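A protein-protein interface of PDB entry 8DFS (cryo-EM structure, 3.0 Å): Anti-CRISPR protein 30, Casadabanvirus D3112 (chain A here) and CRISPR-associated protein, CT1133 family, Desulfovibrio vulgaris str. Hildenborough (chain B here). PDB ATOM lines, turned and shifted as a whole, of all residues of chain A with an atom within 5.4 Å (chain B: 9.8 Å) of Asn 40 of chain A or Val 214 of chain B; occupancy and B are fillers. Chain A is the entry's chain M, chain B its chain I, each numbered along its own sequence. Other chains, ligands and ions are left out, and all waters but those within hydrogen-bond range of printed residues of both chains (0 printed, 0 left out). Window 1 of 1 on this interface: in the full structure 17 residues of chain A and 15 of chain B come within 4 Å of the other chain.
The backbone carbonyl oxygen (O) of Ala 213 of chain B sits at hydrogen-bond distance from the guanidinium group (NH1) of Arg 82 of chain A, 3.1 Å away. The backbone carbonyl oxygen of Gly 203 of chain B is in hydrogen-bond range of the guanidinium group of Arg 82 of chain A, 2.8 Å away. The backbone NH (N) of Ala 213 of chain B lies close to the side-chain amide oxygen (OD1) of Asn 40 of chain A, 3.1 Å away.
O of Ala 213 of chain B lies within hydrogen-bond range of N of Gly 203 of chain B, at 3.1 Å. The side-chain amide oxygen (OE1) of Gln 212 of chain B sits close to the backbone carbonyl oxygen (O) of Ala 361 of chain B (3.2 Å). O of Asn 40 of chain A lies within hydrogen-bond range of N of Ala 55 of chain A, at 2.9 Å. OD1 of Asn 251 of chain B lies within hydrogen-bond range of N of Lys 202 of chain B. The side-chain amide nitrogen (NE2) of Gln 212 of chain B lies close to the backbone carbonyl oxygen (O) of Val 214 of chain B, at 3.3 Å.
Among the printed residues, pairs that only touch across the chains: Arg 82 of chain A with Arg 205 of chain B, Asn 40 of chain A with Gln 212 of chain B, Phe 37 of chain A with Gln 212 of chain B, Arg 82 of chain A with Lys 202 of chain B, Asp 38 of chain A with Gln 212 of chain B, Asn 40 of chain A with Val 214 of chain B and Asp 39 of chain A with Gln 212 of chain B.
Of chain B, only Gln 212, Ala 213 and Val 214 come within 4 Å of Asn 40 of chain A. Of chain A, only Asn 40 comes within 4 Å of Val 214 of chain B. No residue of chain B comes within 4 Å of Ser 41 of chain A. Asp 54 of chain A touches none of the printed residues of chain B. No residue of chain B comes within 4 Å of Ala 55 of chain A. Printed residues of chain B within 4 Å of Asp 38 of chain A: Gln 212 (3.9 Å). Printed residues of chain B within 4 Å of Phe 37 of chain A: Gln 212. Of the printed residues of chain B, Arg 82 of chain A touches Lys 202, Gly 203, Arg 205 and Ala 213. Printed residues of chain A within 4 Å of Ala 213 of chain B: Asn 40 (3.1 Å) and Arg 82 (3.1 Å). Of the printed residues of chain A, Lys 202 of chain B touches Arg 82 (3.6 Å). Ala 362 of chain B touches none of the printed residues of chain A. The nearest residue of chain A that does not touch Val 214 of chain B is Thr 36 of chain A (4.1 Å). The nearest printed residue of chain B that does not touch Arg 82 of chain A is Val 214 of chain B (4.2 Å).
Of the 28 printed residues of chain B, 6 touch a printed residue of chain A. Among the printed residues, 10 pairs touch across the chains.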
ATOM      1  N   ILE A  21      14.459  -5.226 -28.686  1.00  0.00           N
ATOM      2  CA  ILE A  21      13.642  -5.703 -27.574  1.00  0.00           C
ATOM      3  C   ILE A  21      14.366  -6.876 -26.924  1.00  0.00           C
ATOM      4  O   ILE A  21      15.426  -7.300 -27.396  1.00  0.00           O
ATOM      5  CB  ILE A  21      12.214  -6.075 -28.021  1.00  0.00           C
ATOM      6  CG1 ILE A  21      12.143  -7.490 -28.609  1.00  0.00           C
ATOM      7  CG2 ILE A  21      11.694  -5.056 -29.022  1.00  0.00           C
ATOM      8  CD1 ILE A  21      10.728  -7.957 -28.869  1.00  0.00           C
ATOM      9  N   THR A  36      16.667  -9.689 -30.248  1.00  0.00           N
ATOM     10  CA  THR A  36      15.377  -9.810 -30.906  1.00  0.00           C
ATOM     11  C   THR A  36      14.741  -8.435 -31.047  1.00  0.00           C
ATOM     12  O   THR A  36      14.942  -7.550 -30.212  1.00  0.00           O
ATOM     13  CB  THR A  36      14.440 -10.734 -30.126  1.00  0.00           C
ATOM     14  OG1 THR A  36      13.996 -10.074 -28.934  1.00  0.00           O
ATOM     15  CG2 THR A  36      15.151 -12.024 -29.753  1.00  0.00           C
ATOM     16  N   PHE A  37      13.973  -8.266 -32.118  1.00  0.00           N
ATOM     17  CA  PHE A  37      13.299  -7.015 -32.423  1.00  0.00           C
ATOM     18  C   PHE A  37      11.827  -7.301 -32.675  1.00  0.00           C
ATOM     19  O   PHE A  37      11.388  -8.455 -32.698  1.00  0.00           O
ATOM     20  CB  PHE A  37      13.920  -6.333 -33.649  1.00  0.00           C
ATOM     21  CG  PHE A  37      15.408  -6.167 -33.568  1.00  0.00           C
ATOM     22  CD1 PHE A  37      16.251  -7.226 -33.846  1.00  0.00           C
ATOM     23  CD2 PHE A  37      15.964  -4.948 -33.231  1.00  0.00           C
ATOM     24  CE1 PHE A  37      17.619  -7.076 -33.776  1.00  0.00           C
ATOM     25  CE2 PHE A  37      17.333  -4.792 -33.161  1.00  0.00           C
ATOM     26  CZ  PHE A  37      18.160  -5.857 -33.435  1.00  0.00           C
ATOM     27  N   ASP A  38      11.055  -6.235 -32.862  1.00  0.00           N
ATOM     28  CA  ASP A  38       9.715  -6.387 -33.401  1.00  0.00           C
ATOM     29  C   ASP A  38       9.809  -6.904 -34.836  1.00  0.00           C
ATOM     30  O   ASP A  38      10.897  -7.080 -35.392  1.00  0.00           O
ATOM     31  CB  ASP A  38       8.954  -5.063 -33.335  1.00  0.00           C
ATOM     32  CG  ASP A  38       9.814  -3.875 -33.716  1.00  0.00           C
ATOM     33  OD1 ASP A  38      11.018  -3.886 -33.388  1.00  0.00           O
ATOM     34  OD2 ASP A  38       9.287  -2.931 -34.342  1.00  0.00           O
ATOM     35  N   ASP A  39       8.655  -7.156 -35.445  1.00  0.00           N
ATOM     36  CA  ASP A  39       8.586  -7.717 -36.792  1.00  0.00           C
ATOM     37  C   ASP A  39       9.136  -9.137 -36.849  1.00  0.00           C
ATOM     38  O   ASP A  39       9.449  -9.641 -37.932  1.00  0.00           O
ATOM     39  CB  ASP A  39       9.325  -6.832 -37.802  1.00  0.00           C
ATOM     40  CG  ASP A  39       8.979  -5.365 -37.661  1.00  0.00           C
ATOM     41  OD1 ASP A  39       9.366  -4.754 -36.644  1.00  0.00           O
ATOM     42  OD2 ASP A  39       8.320  -4.820 -38.571  1.00  0.00           O
ATOM     43  N   ASN A  40       9.261  -9.798 -35.698  1.00  0.00           N
ATOM     44  CA  ASN A  40       9.703 -11.191 -35.640  1.00  0.00           C
ATOM     45  C   ASN A  40      11.082 -11.365 -36.275  1.00  0.00           C
ATOM     46  O   ASN A  40      11.375 -12.385 -36.901  1.00  0.00           O
ATOM     47  CB  ASN A  40       8.675 -12.110 -36.306  1.00  0.00           C
ATOM     48  CG  ASN A  40       7.989 -13.032 -35.321  1.00  0.00           C
ATOM     49  OD1 ASN A  40       8.536 -13.354 -34.267  1.00  0.00           O
ATOM     50  ND2 ASN A  40       6.782 -13.466 -35.664  1.00  0.00           N
ATOM     51  N   SER A  41      11.944 -10.367 -36.099  1.00  0.00           N
ATOM     52  CA  SER A  41      13.300 -10.391 -36.627  1.00  0.00           C
ATOM     53  C   SER A  41      14.293 -10.463 -35.476  1.00  0.00           C
ATOM     54  O   SER A  41      14.136  -9.771 -34.466  1.00  0.00           O
ATOM     55  CB  SER A  41      13.582  -9.155 -37.481  1.00  0.00           C
ATOM     56  OG  SER A  41      14.814  -9.284 -38.166  1.00  0.00           O
ATOM     57  N   VAL A  42      15.312 -11.304 -35.632  1.00  0.00           N
ATOM     58  CA  VAL A  42      16.297 -11.559 -34.588  1.00  0.00           C
ATOM     59  C   VAL A  42      17.689 -11.429 -35.188  1.00  0.00           C
ATOM     60  O   VAL A  42      17.936 -11.908 -36.301  1.00  0.00           O
ATOM     61  CB  VAL A  42      16.113 -12.955 -33.963  1.00  0.00           C
ATOM     62  CG1 VAL A  42      17.160 -13.197 -32.886  1.00  0.00           C
ATOM     63  CG2 VAL A  42      14.709 -13.101 -33.400  1.00  0.00           C
ATOM     64  N   MET A  53      18.155 -13.399 -39.008  1.00  0.00           N
ATOM     65  CA  MET A  53      17.137 -14.430 -39.134  1.00  0.00           C
ATOM     66  C   MET A  53      15.753 -13.801 -39.114  1.00  0.00           C
ATOM     67  O   MET A  53      15.517 -12.813 -38.414  1.00  0.00           O
ATOM     68  CB  MET A  53      17.254 -15.455 -38.001  1.00  0.00           C
ATOM     69  CG  MET A  53      16.404 -16.699 -38.206  1.00  0.00           C
ATOM     70  SD  MET A  53      14.885 -16.704 -37.233  1.00  0.00           S
ATOM     71  CE  MET A  53      15.536 -16.585 -35.571  1.00  0.00           C
ATOM     72  N   ASP A  54      14.842 -14.380 -39.891  1.00  0.00           N
ATOM     73  CA  ASP A  54      13.439 -13.994 -39.898  1.00  0.00           C
ATOM     74  C   ASP A  54      12.618 -15.153 -39.352  1.00  0.00           C
ATOM     75  O   ASP A  54      12.822 -16.304 -39.752  1.00  0.00           O
ATOM     76  CB  ASP A  54      12.975 -13.627 -41.308  1.00  0.00           C
ATOM     77  CG  ASP A  54      11.598 -12.996 -41.321  1.00  0.00           C
ATOM     78  OD1 ASP A  54      10.826 -13.232 -40.368  1.00  0.00           O
ATOM     79  OD2 ASP A  54      11.286 -12.263 -42.282  1.00  0.00           O
ATOM     80  N   ALA A  55      11.694 -14.849 -38.446  1.00  0.00           N
ATOM     81  CA  ALA A  55      10.966 -15.881 -37.719  1.00  0.00           C
ATOM     82  C   ALA A  55       9.688 -16.327 -38.417  1.00  0.00           C
ATOM     83  O   ALA A  55       8.944 -17.130 -37.845  1.00  0.00           O
ATOM     84  CB  ALA A  55      10.629 -15.386 -36.310  1.00  0.00           C
ATOM     85  N   ASP A  56       9.409 -15.835 -39.622  1.00  0.00           N
ATOM     86  CA  ASP A  56       8.217 -16.226 -40.363  1.00  0.00           C
ATOM     87  C   ASP A  56       8.536 -17.030 -41.616  1.00  0.00           C
ATOM     88  O   ASP A  56       7.616 -17.578 -42.232  1.00  0.00           O
ATOM     89  CB  ASP A  56       7.398 -14.987 -40.745  1.00  0.00           C
ATOM     90  CG  ASP A  56       8.256 -13.872 -41.305  1.00  0.00           C
ATOM     91  OD1 ASP A  56       9.111 -14.159 -42.167  1.00  0.00           O
ATOM     92  OD2 ASP A  56       8.079 -12.711 -40.879  1.00  0.00           O
ATOM     93  N   ARG A  82      10.283 -24.725 -32.676  1.00  0.00           N
ATOM     94  CA  ARG A  82       9.233 -23.783 -32.304  1.00  0.00           C
ATOM     95  C   ARG A  82       8.976 -22.779 -33.421  1.00  0.00           C
ATOM     96  O   ARG A  82       7.829 -22.567 -33.829  1.00  0.00           O
ATOM     97  CB  ARG A  82       9.615 -23.064 -31.011  1.00  0.00           C
ATOM     98  CG  ARG A  82       8.428 -22.580 -30.194  1.00  0.00           C
ATOM     99  CD  ARG A  82       8.865 -21.959 -28.878  1.00  0.00           C
ATOM    100  NE  ARG A  82       9.788 -20.849 -29.075  1.00  0.00           N
ATOM    101  CZ  ARG A  82       9.419 -19.607 -29.355  1.00  0.00           C
ATOM    102  NH1 ARG A  82       8.146 -19.277 -29.491  1.00  0.00           N
ATOM    103  NH2 ARG A  82      10.352 -18.672 -29.507  1.00  0.00           N
ATOM    104  N   HIS B 198      15.982  -7.552 -20.979  1.00  0.00           N
ATOM    105  CA  HIS B 198      15.495  -8.780 -20.367  1.00  0.00           C
ATOM    106  C   HIS B 198      15.589  -9.927 -21.356  1.00  0.00           C
ATOM    107  O   HIS B 198      15.750  -9.723 -22.559  1.00  0.00           O
ATOM    108  CB  HIS B 198      14.056  -8.587 -19.904  1.00  0.00           C
ATOM    109  CG  HIS B 198      13.922  -7.710 -18.699  1.00  0.00           C
ATOM    110  ND1 HIS B 198      13.022  -7.969 -17.689  1.00  0.00           N
ATOM    111  CD2 HIS B 198      14.576  -6.580 -18.341  1.00  0.00           C
ATOM    112  CE1 HIS B 198      13.124  -7.034 -16.762  1.00  0.00           C
ATOM    113  NE2 HIS B 198      14.061  -6.180 -17.134  1.00  0.00           N
ATOM    114  N   PRO B 199      15.542 -11.166 -20.877  1.00  0.00           N
ATOM    115  CA  PRO B 199      15.351 -12.298 -21.788  1.00  0.00           C
ATOM    116  C   PRO B 199      13.919 -12.372 -22.289  1.00  0.00           C
ATOM    117  O   PRO B 199      12.964 -12.053 -21.577  1.00  0.00           O
ATOM    118  CB  PRO B 199      15.709 -13.516 -20.928  1.00  0.00           C
ATOM    119  CG  PRO B 199      15.602 -13.058 -19.530  1.00  0.00           C
ATOM    120  CD  PRO B 199      15.887 -11.598 -19.515  1.00  0.00           C
ATOM    121  N   SER B 200      13.778 -12.806 -23.537  1.00  0.00           N
ATOM    122  CA  SER B 200      12.485 -12.790 -24.201  1.00  0.00           C
ATOM    123  C   SER B 200      11.585 -13.901 -23.665  1.00  0.00           C
ATOM    124  O   SER B 200      12.026 -14.822 -22.973  1.00  0.00           O
ATOM    125  CB  SER B 200      12.659 -12.933 -25.712  1.00  0.00           C
ATOM    126  OG  SER B 200      13.358 -14.120 -26.033  1.00  0.00           O
ATOM    127  N   ILE B 201      10.301 -13.800 -24.000  1.00  0.00           N
ATOM    128  CA  ILE B 201       9.281 -14.741 -23.558  1.00  0.00           C
ATOM    129  C   ILE B 201       8.720 -15.457 -24.776  1.00  0.00           C
ATOM    130  O   ILE B 201       8.507 -14.843 -25.826  1.00  0.00           O
ATOM    131  CB  ILE B 201       8.159 -14.029 -22.773  1.00  0.00           C
ATOM    132  CG1 ILE B 201       8.586 -13.825 -21.322  1.00  0.00           C
ATOM    133  CG2 ILE B 201       6.864 -14.829 -22.830  1.00  0.00           C
ATOM    134  CD1 ILE B 201       7.763 -12.804 -20.583  1.00  0.00           C
ATOM    135  N   LYS B 202       8.483 -16.757 -24.631  1.00  0.00           N
ATOM    136  CA  LYS B 202       7.966 -17.553 -25.734  1.00  0.00           C
ATOM    137  C   LYS B 202       6.604 -17.038 -26.177  1.00  0.00           C
ATOM    138  O   LYS B 202       5.803 -16.567 -25.365  1.00  0.00           O
ATOM    139  CB  LYS B 202       7.853 -19.020 -25.323  1.00  0.00           C
ATOM    140  CG  LYS B 202       9.053 -19.869 -25.694  1.00  0.00           C
ATOM    141  CD  LYS B 202      10.223 -19.608 -24.763  1.00  0.00           C
ATOM    142  CE  LYS B 202      11.392 -20.526 -25.068  1.00  0.00           C
ATOM    143  NZ  LYS B 202      12.569 -20.231 -24.207  1.00  0.00           N
ATOM    144  N   GLY B 203       6.346 -17.125 -27.481  1.00  0.00           N
ATOM    145  CA  GLY B 203       5.047 -16.804 -28.021  1.00  0.00           C
ATOM    146  C   GLY B 203       4.645 -17.810 -29.081  1.00  0.00           C
ATOM    147  O   GLY B 203       5.478 -18.337 -29.819  1.00  0.00           O
ATOM    148  N   GLY B 204       3.348 -18.066 -29.147  1.00  0.00           N
ATOM    149  CA  GLY B 204       2.801 -19.013 -30.104  1.00  0.00           C
ATOM    150  C   GLY B 204       2.245 -20.252 -29.413  1.00  0.00           C
ATOM    151  O   GLY B 204       1.458 -20.146 -28.475  1.00  0.00           O
ATOM    152  N   ARG B 205       2.660 -21.430 -29.885  1.00  0.00           N
ATOM    153  CA  ARG B 205       2.075 -22.672 -29.389  1.00  0.00           C
ATOM    154  C   ARG B 205       2.377 -22.885 -27.910  1.00  0.00           C
ATOM    155  O   ARG B 205       1.494 -23.296 -27.147  1.00  0.00           O
ATOM    156  CB  ARG B 205       2.582 -23.854 -30.215  1.00  0.00           C
ATOM    157  CG  ARG B 205       3.995 -24.300 -29.873  1.00  0.00           C
ATOM    158  CD  ARG B 205       4.700 -24.912 -31.061  1.00  0.00           C
ATOM    159  NE  ARG B 205       6.136 -25.036 -30.842  1.00  0.00           N
ATOM    160  CZ  ARG B 205       6.695 -25.889 -29.993  1.00  0.00           C
ATOM    161  NH1 ARG B 205       5.965 -26.712 -29.257  1.00  0.00           N
ATOM    162  NH2 ARG B 205       8.020 -25.917 -29.878  1.00  0.00           N
ATOM    163  N   GLY B 207       3.753 -20.397 -25.935  1.00  0.00           N
ATOM    164  CA  GLY B 207       3.801 -19.112 -25.272  1.00  0.00           C
ATOM    165  C   GLY B 207       2.418 -18.514 -25.166  1.00  0.00           C
ATOM    166  O   GLY B 207       1.419 -19.237 -25.224  1.00  0.00           O
ATOM    167  N   VAL B 208       2.337 -17.195 -25.012  1.00  0.00           N
ATOM    168  CA  VAL B 208       1.041 -16.530 -24.980  1.00  0.00           C
ATOM    169  C   VAL B 208       0.454 -16.601 -26.385  1.00  0.00           C
ATOM    170  O   VAL B 208       0.921 -15.914 -27.298  1.00  0.00           O
ATOM    171  CB  VAL B 208       1.161 -15.083 -24.497  1.00  0.00           C
ATOM    172  CG1 VAL B 208      -0.103 -14.316 -24.829  1.00  0.00           C
ATOM    173  CG2 VAL B 208       1.436 -15.049 -23.005  1.00  0.00           C
ATOM    174  N   GLY B 210      -1.229 -15.994 -29.668  1.00  0.00           N
ATOM    175  CA  GLY B 210      -1.555 -14.753 -30.335  1.00  0.00           C
ATOM    176  C   GLY B 210      -0.365 -13.832 -30.514  1.00  0.00           C
ATOM    177  O   GLY B 210      -0.273 -13.146 -31.539  1.00  0.00           O
ATOM    178  N   ALA B 211       0.543 -13.801 -29.544  1.00  0.00           N
ATOM    179  CA  ALA B 211       1.738 -12.984 -29.657  1.00  0.00           C
ATOM    180  C   ALA B 211       2.703 -13.595 -30.664  1.00  0.00           C
ATOM    181  O   ALA B 211       2.671 -14.795 -30.947  1.00  0.00           O
ATOM    182  CB  ALA B 211       2.425 -12.839 -28.302  1.00  0.00           C
ATOM    183  N   GLN B 212       3.575 -12.751 -31.206  1.00  0.00           N
ATOM    184  CA  GLN B 212       4.551 -13.220 -32.172  1.00  0.00           C
ATOM    185  C   GLN B 212       5.555 -14.145 -31.483  1.00  0.00           C
ATOM    186  O   GLN B 212       5.500 -14.381 -30.274  1.00  0.00           O
ATOM    187  CB  GLN B 212       5.233 -12.035 -32.849  1.00  0.00           C
ATOM    188  CG  GLN B 212       6.471 -11.521 -32.148  1.00  0.00           C
ATOM    189  CD  GLN B 212       6.888 -10.157 -32.658  1.00  0.00           C
ATOM    190  OE1 GLN B 212       6.160  -9.517 -33.417  1.00  0.00           O
ATOM    191  NE2 GLN B 212       8.068  -9.706 -32.250  1.00  0.00           N
ATOM    192  N   ALA B 213       6.489 -14.679 -32.273  1.00  0.00           N
ATOM    193  CA  ALA B 213       7.348 -15.753 -31.784  1.00  0.00           C
ATOM    194  C   ALA B 213       8.092 -15.363 -30.515  1.00  0.00           C
ATOM    195  O   ALA B 213       8.366 -16.224 -29.672  1.00  0.00           O
ATOM    196  CB  ALA B 213       8.340 -16.163 -32.870  1.00  0.00           C
ATOM    197  N   VAL B 214       8.432 -14.086 -30.357  1.00  0.00           N
ATOM    198  CA  VAL B 214       9.165 -13.605 -29.192  1.00  0.00           C
ATOM    199  C   VAL B 214       8.472 -12.358 -28.664  1.00  0.00           C
ATOM    200  O   VAL B 214       8.142 -11.453 -29.438  1.00  0.00           O
ATOM    201  CB  VAL B 214      10.640 -13.306 -29.525  1.00  0.00           C
ATOM    202  CG1 VAL B 214      11.402 -14.598 -29.758  1.00  0.00           C
ATOM    203  CG2 VAL B 214      10.748 -12.389 -30.735  1.00  0.00           C
ATOM    204  N   ALA B 215       8.255 -12.311 -27.351  1.00  0.00           N
ATOM    205  CA  ALA B 215       7.588 -11.191 -26.705  1.00  0.00           C
ATOM    206  C   ALA B 215       8.274 -10.907 -25.377  1.00  0.00           C
ATOM    207  O   ALA B 215       9.169 -11.640 -24.949  1.00  0.00           O
ATOM    208  CB  ALA B 215       6.097 -11.474 -26.492  1.00  0.00           C
ATOM    209  N   SER B 216       7.848  -9.831 -24.719  1.00  0.00           N
ATOM    210  CA  SER B 216       8.475  -9.414 -23.473  1.00  0.00           C
ATOM    211  C   SER B 216       7.480  -8.642 -22.621  1.00  0.00           C
ATOM    212  O   SER B 216       6.662  -7.876 -23.135  1.00  0.00           O
ATOM    213  CB  SER B 216       9.706  -8.543 -23.736  1.00  0.00           C
ATOM    214  OG  SER B 216      10.537  -9.127 -24.721  1.00  0.00           O
ATOM    215  N   ILE B 217       7.569  -8.847 -21.306  1.00  0.00           N
ATOM    216  CA  ILE B 217       6.789  -8.038 -20.373  1.00  0.00           C
ATOM    217  C   ILE B 217       7.216  -6.580 -20.457  1.00  0.00           C
ATOM    218  O   ILE B 217       6.380  -5.673 -20.540  1.00  0.00           O
ATOM    219  CB  ILE B 217       6.941  -8.577 -18.939  1.00  0.00           C
ATOM    220  CG1 ILE B 217       6.403 -10.002 -18.818  1.00  0.00           C
ATOM    221  CG2 ILE B 217       6.229  -7.662 -17.955  1.00  0.00           C
ATOM    222  CD1 ILE B 217       4.913 -10.128 -19.015  1.00  0.00           C
ATOM    223  N   VAL B 218       8.523  -6.335 -20.439  1.00  0.00           N
ATOM    224  CA  VAL B 218       9.083  -4.990 -20.390  1.00  0.00           C
ATOM    225  C   VAL B 218       9.734  -4.679 -21.728  1.00  0.00           C
ATOM    226  O   VAL B 218      10.523  -5.473 -22.249  1.00  0.00           O
ATOM    227  CB  VAL B 218      10.095  -4.845 -19.238  1.00  0.00           C
ATOM    228  CG1 VAL B 218       9.532  -5.441 -17.961  1.00  0.00           C
ATOM    229  CG2 VAL B 218      11.410  -5.505 -19.595  1.00  0.00           C
ATOM    230  N   SER B 219       9.393  -3.520 -22.287  1.00  0.00           N
ATOM    231  CA  SER B 219       9.947  -3.095 -23.564  1.00  0.00           C
ATOM    232  C   SER B 219       9.823  -1.584 -23.657  1.00  0.00           C
ATOM    233  O   SER B 219       8.767  -1.031 -23.339  1.00  0.00           O
ATOM    234  CB  SER B 219       9.218  -3.766 -24.731  1.00  0.00           C
ATOM    235  OG  SER B 219       9.132  -5.166 -24.539  1.00  0.00           O
ATOM    236  N   ASN B 251       8.299 -18.771 -18.701  1.00  0.00           N
ATOM    237  CA  ASN B 251       8.430 -19.674 -19.840  1.00  0.00           C
ATOM    238  C   ASN B 251       8.105 -21.107 -19.446  1.00  0.00           C
ATOM    239  O   ASN B 251       7.434 -21.827 -20.195  1.00  0.00           O
ATOM    240  CB  ASN B 251       9.839 -19.586 -20.420  1.00  0.00           C
ATOM    241  CG  ASN B 251       9.990 -18.453 -21.412  1.00  0.00           C
ATOM    242  OD1 ASN B 251       9.052 -18.113 -22.130  1.00  0.00           O
ATOM    243  ND2 ASN B 251      11.177 -17.863 -21.459  1.00  0.00           N
ATOM    244  N   LEU B 254       4.447 -21.454 -19.216  1.00  0.00           N
ATOM    245  CA  LEU B 254       3.793 -21.355 -20.513  1.00  0.00           C
ATOM    246  C   LEU B 254       3.939 -22.613 -21.358  1.00  0.00           C
ATOM    247  O   LEU B 254       3.280 -22.713 -22.398  1.00  0.00           O
ATOM    248  CB  LEU B 254       4.349 -20.157 -21.284  1.00  0.00           C
ATOM    249  CG  LEU B 254       3.893 -18.784 -20.792  1.00  0.00           C
ATOM    250  CD1 LEU B 254       4.654 -17.683 -21.504  1.00  0.00           C
ATOM    251  CD2 LEU B 254       2.399 -18.607 -20.991  1.00  0.00           C
ATOM    252  N   PRO B 359      -2.080 -10.752 -25.526  1.00  0.00           N
ATOM    253  CA  PRO B 359      -1.014 -10.334 -26.441  1.00  0.00           C
ATOM    254  C   PRO B 359      -1.385  -9.186 -27.361  1.00  0.00           C
ATOM    255  O   PRO B 359      -2.563  -8.871 -27.548  1.00  0.00           O
ATOM    256  CB  PRO B 359      -0.761 -11.607 -27.248  1.00  0.00           C
ATOM    257  CG  PRO B 359      -2.126 -12.197 -27.378  1.00  0.00           C
ATOM    258  CD  PRO B 359      -2.868 -11.856 -26.100  1.00  0.00           C
ATOM    259  N   ASN B 360      -0.367  -8.563 -27.941  1.00  0.00           N
ATOM    260  CA  ASN B 360      -0.531  -7.696 -29.101  1.00  0.00           C
ATOM    261  C   ASN B 360       0.661  -7.968 -30.014  1.00  0.00           C
ATOM    262  O   ASN B 360       1.356  -8.980 -29.865  1.00  0.00           O
ATOM    263  CB  ASN B 360      -0.687  -6.223 -28.689  1.00  0.00           C
ATOM    264  CG  ASN B 360       0.538  -5.670 -28.012  1.00  0.00           C
ATOM    265  OD1 ASN B 360       1.640  -5.734 -28.551  1.00  0.00           O
ATOM    266  ND2 ASN B 360       0.352  -5.110 -26.824  1.00  0.00           N
ATOM    267  N   ALA B 361       0.898  -7.070 -30.972  1.00  0.00           N
ATOM    268  CA  ALA B 361       1.831  -7.349 -32.061  1.00  0.00           C
ATOM    269  C   ALA B 361       3.079  -8.081 -31.577  1.00  0.00           C
ATOM    270  O   ALA B 361       3.351  -9.210 -31.998  1.00  0.00           O
ATOM    271  CB  ALA B 361       2.219  -6.044 -32.756  1.00  0.00           C
ATOM    272  N   ALA B 362       3.846  -7.457 -30.683  1.00  0.00           N
ATOM    273  CA  ALA B 362       5.103  -8.041 -30.235  1.00  0.00           C
ATOM    274  C   ALA B 362       5.287  -8.023 -28.726  1.00  0.00           C
ATOM    275  O   ALA B 362       6.223  -8.660 -28.234  1.00  0.00           O
ATOM    276  CB  ALA B 362       6.287  -7.315 -30.892  1.00  0.00           C
ATOM    277  N   ARG B 363       4.440  -7.322 -27.979  1.00  0.00           N
ATOM    278  CA  ARG B 363       4.532  -7.279 -26.529  1.00  0.00           C
ATOM    279  C   ARG B 363       3.191  -7.679 -25.941  1.00  0.00           C
ATOM    280  O   ARG B 363       2.134  -7.420 -26.520  1.00  0.00           O
ATOM    281  CB  ARG B 363       4.950  -5.888 -26.040  1.00  0.00           C
ATOM    282  CG  ARG B 363       3.801  -4.907 -25.893  1.00  0.00           C
ATOM    283  CD  ARG B 363       4.250  -3.476 -26.139  1.00  0.00           C
ATOM    284  NE  ARG B 363       3.125  -2.616 -26.481  1.00  0.00           N
ATOM    285  CZ  ARG B 363       3.171  -1.615 -27.350  1.00  0.00           C
ATOM    286  NH1 ARG B 363       4.286  -1.303 -27.993  1.00  0.00           N
ATOM    287  NH2 ARG B 363       2.070  -0.908 -27.583  1.00  0.00           N
ATOM    288  N   LEU B 364       3.242  -8.322 -24.780  1.00  0.00           N
ATOM    289  CA  LEU B 364       2.057  -8.871 -24.144  1.00  0.00           C
ATOM    290  C   LEU B 364       1.816  -8.170 -22.815  1.00  0.00           C
ATOM    291  O   LEU B 364       2.757  -7.801 -22.110  1.00  0.00           O
ATOM    292  CB  LEU B 364       2.191 -10.387 -23.953  1.00  0.00           C
ATOM    293  CG  LEU B 364       3.549 -10.917 -23.492  1.00  0.00           C
ATOM    294  CD1 LEU B 364       3.835 -10.529 -22.055  1.00  0.00           C
ATOM    295  CD2 LEU B 364       3.616 -12.418 -23.672  1.00  0.00           C
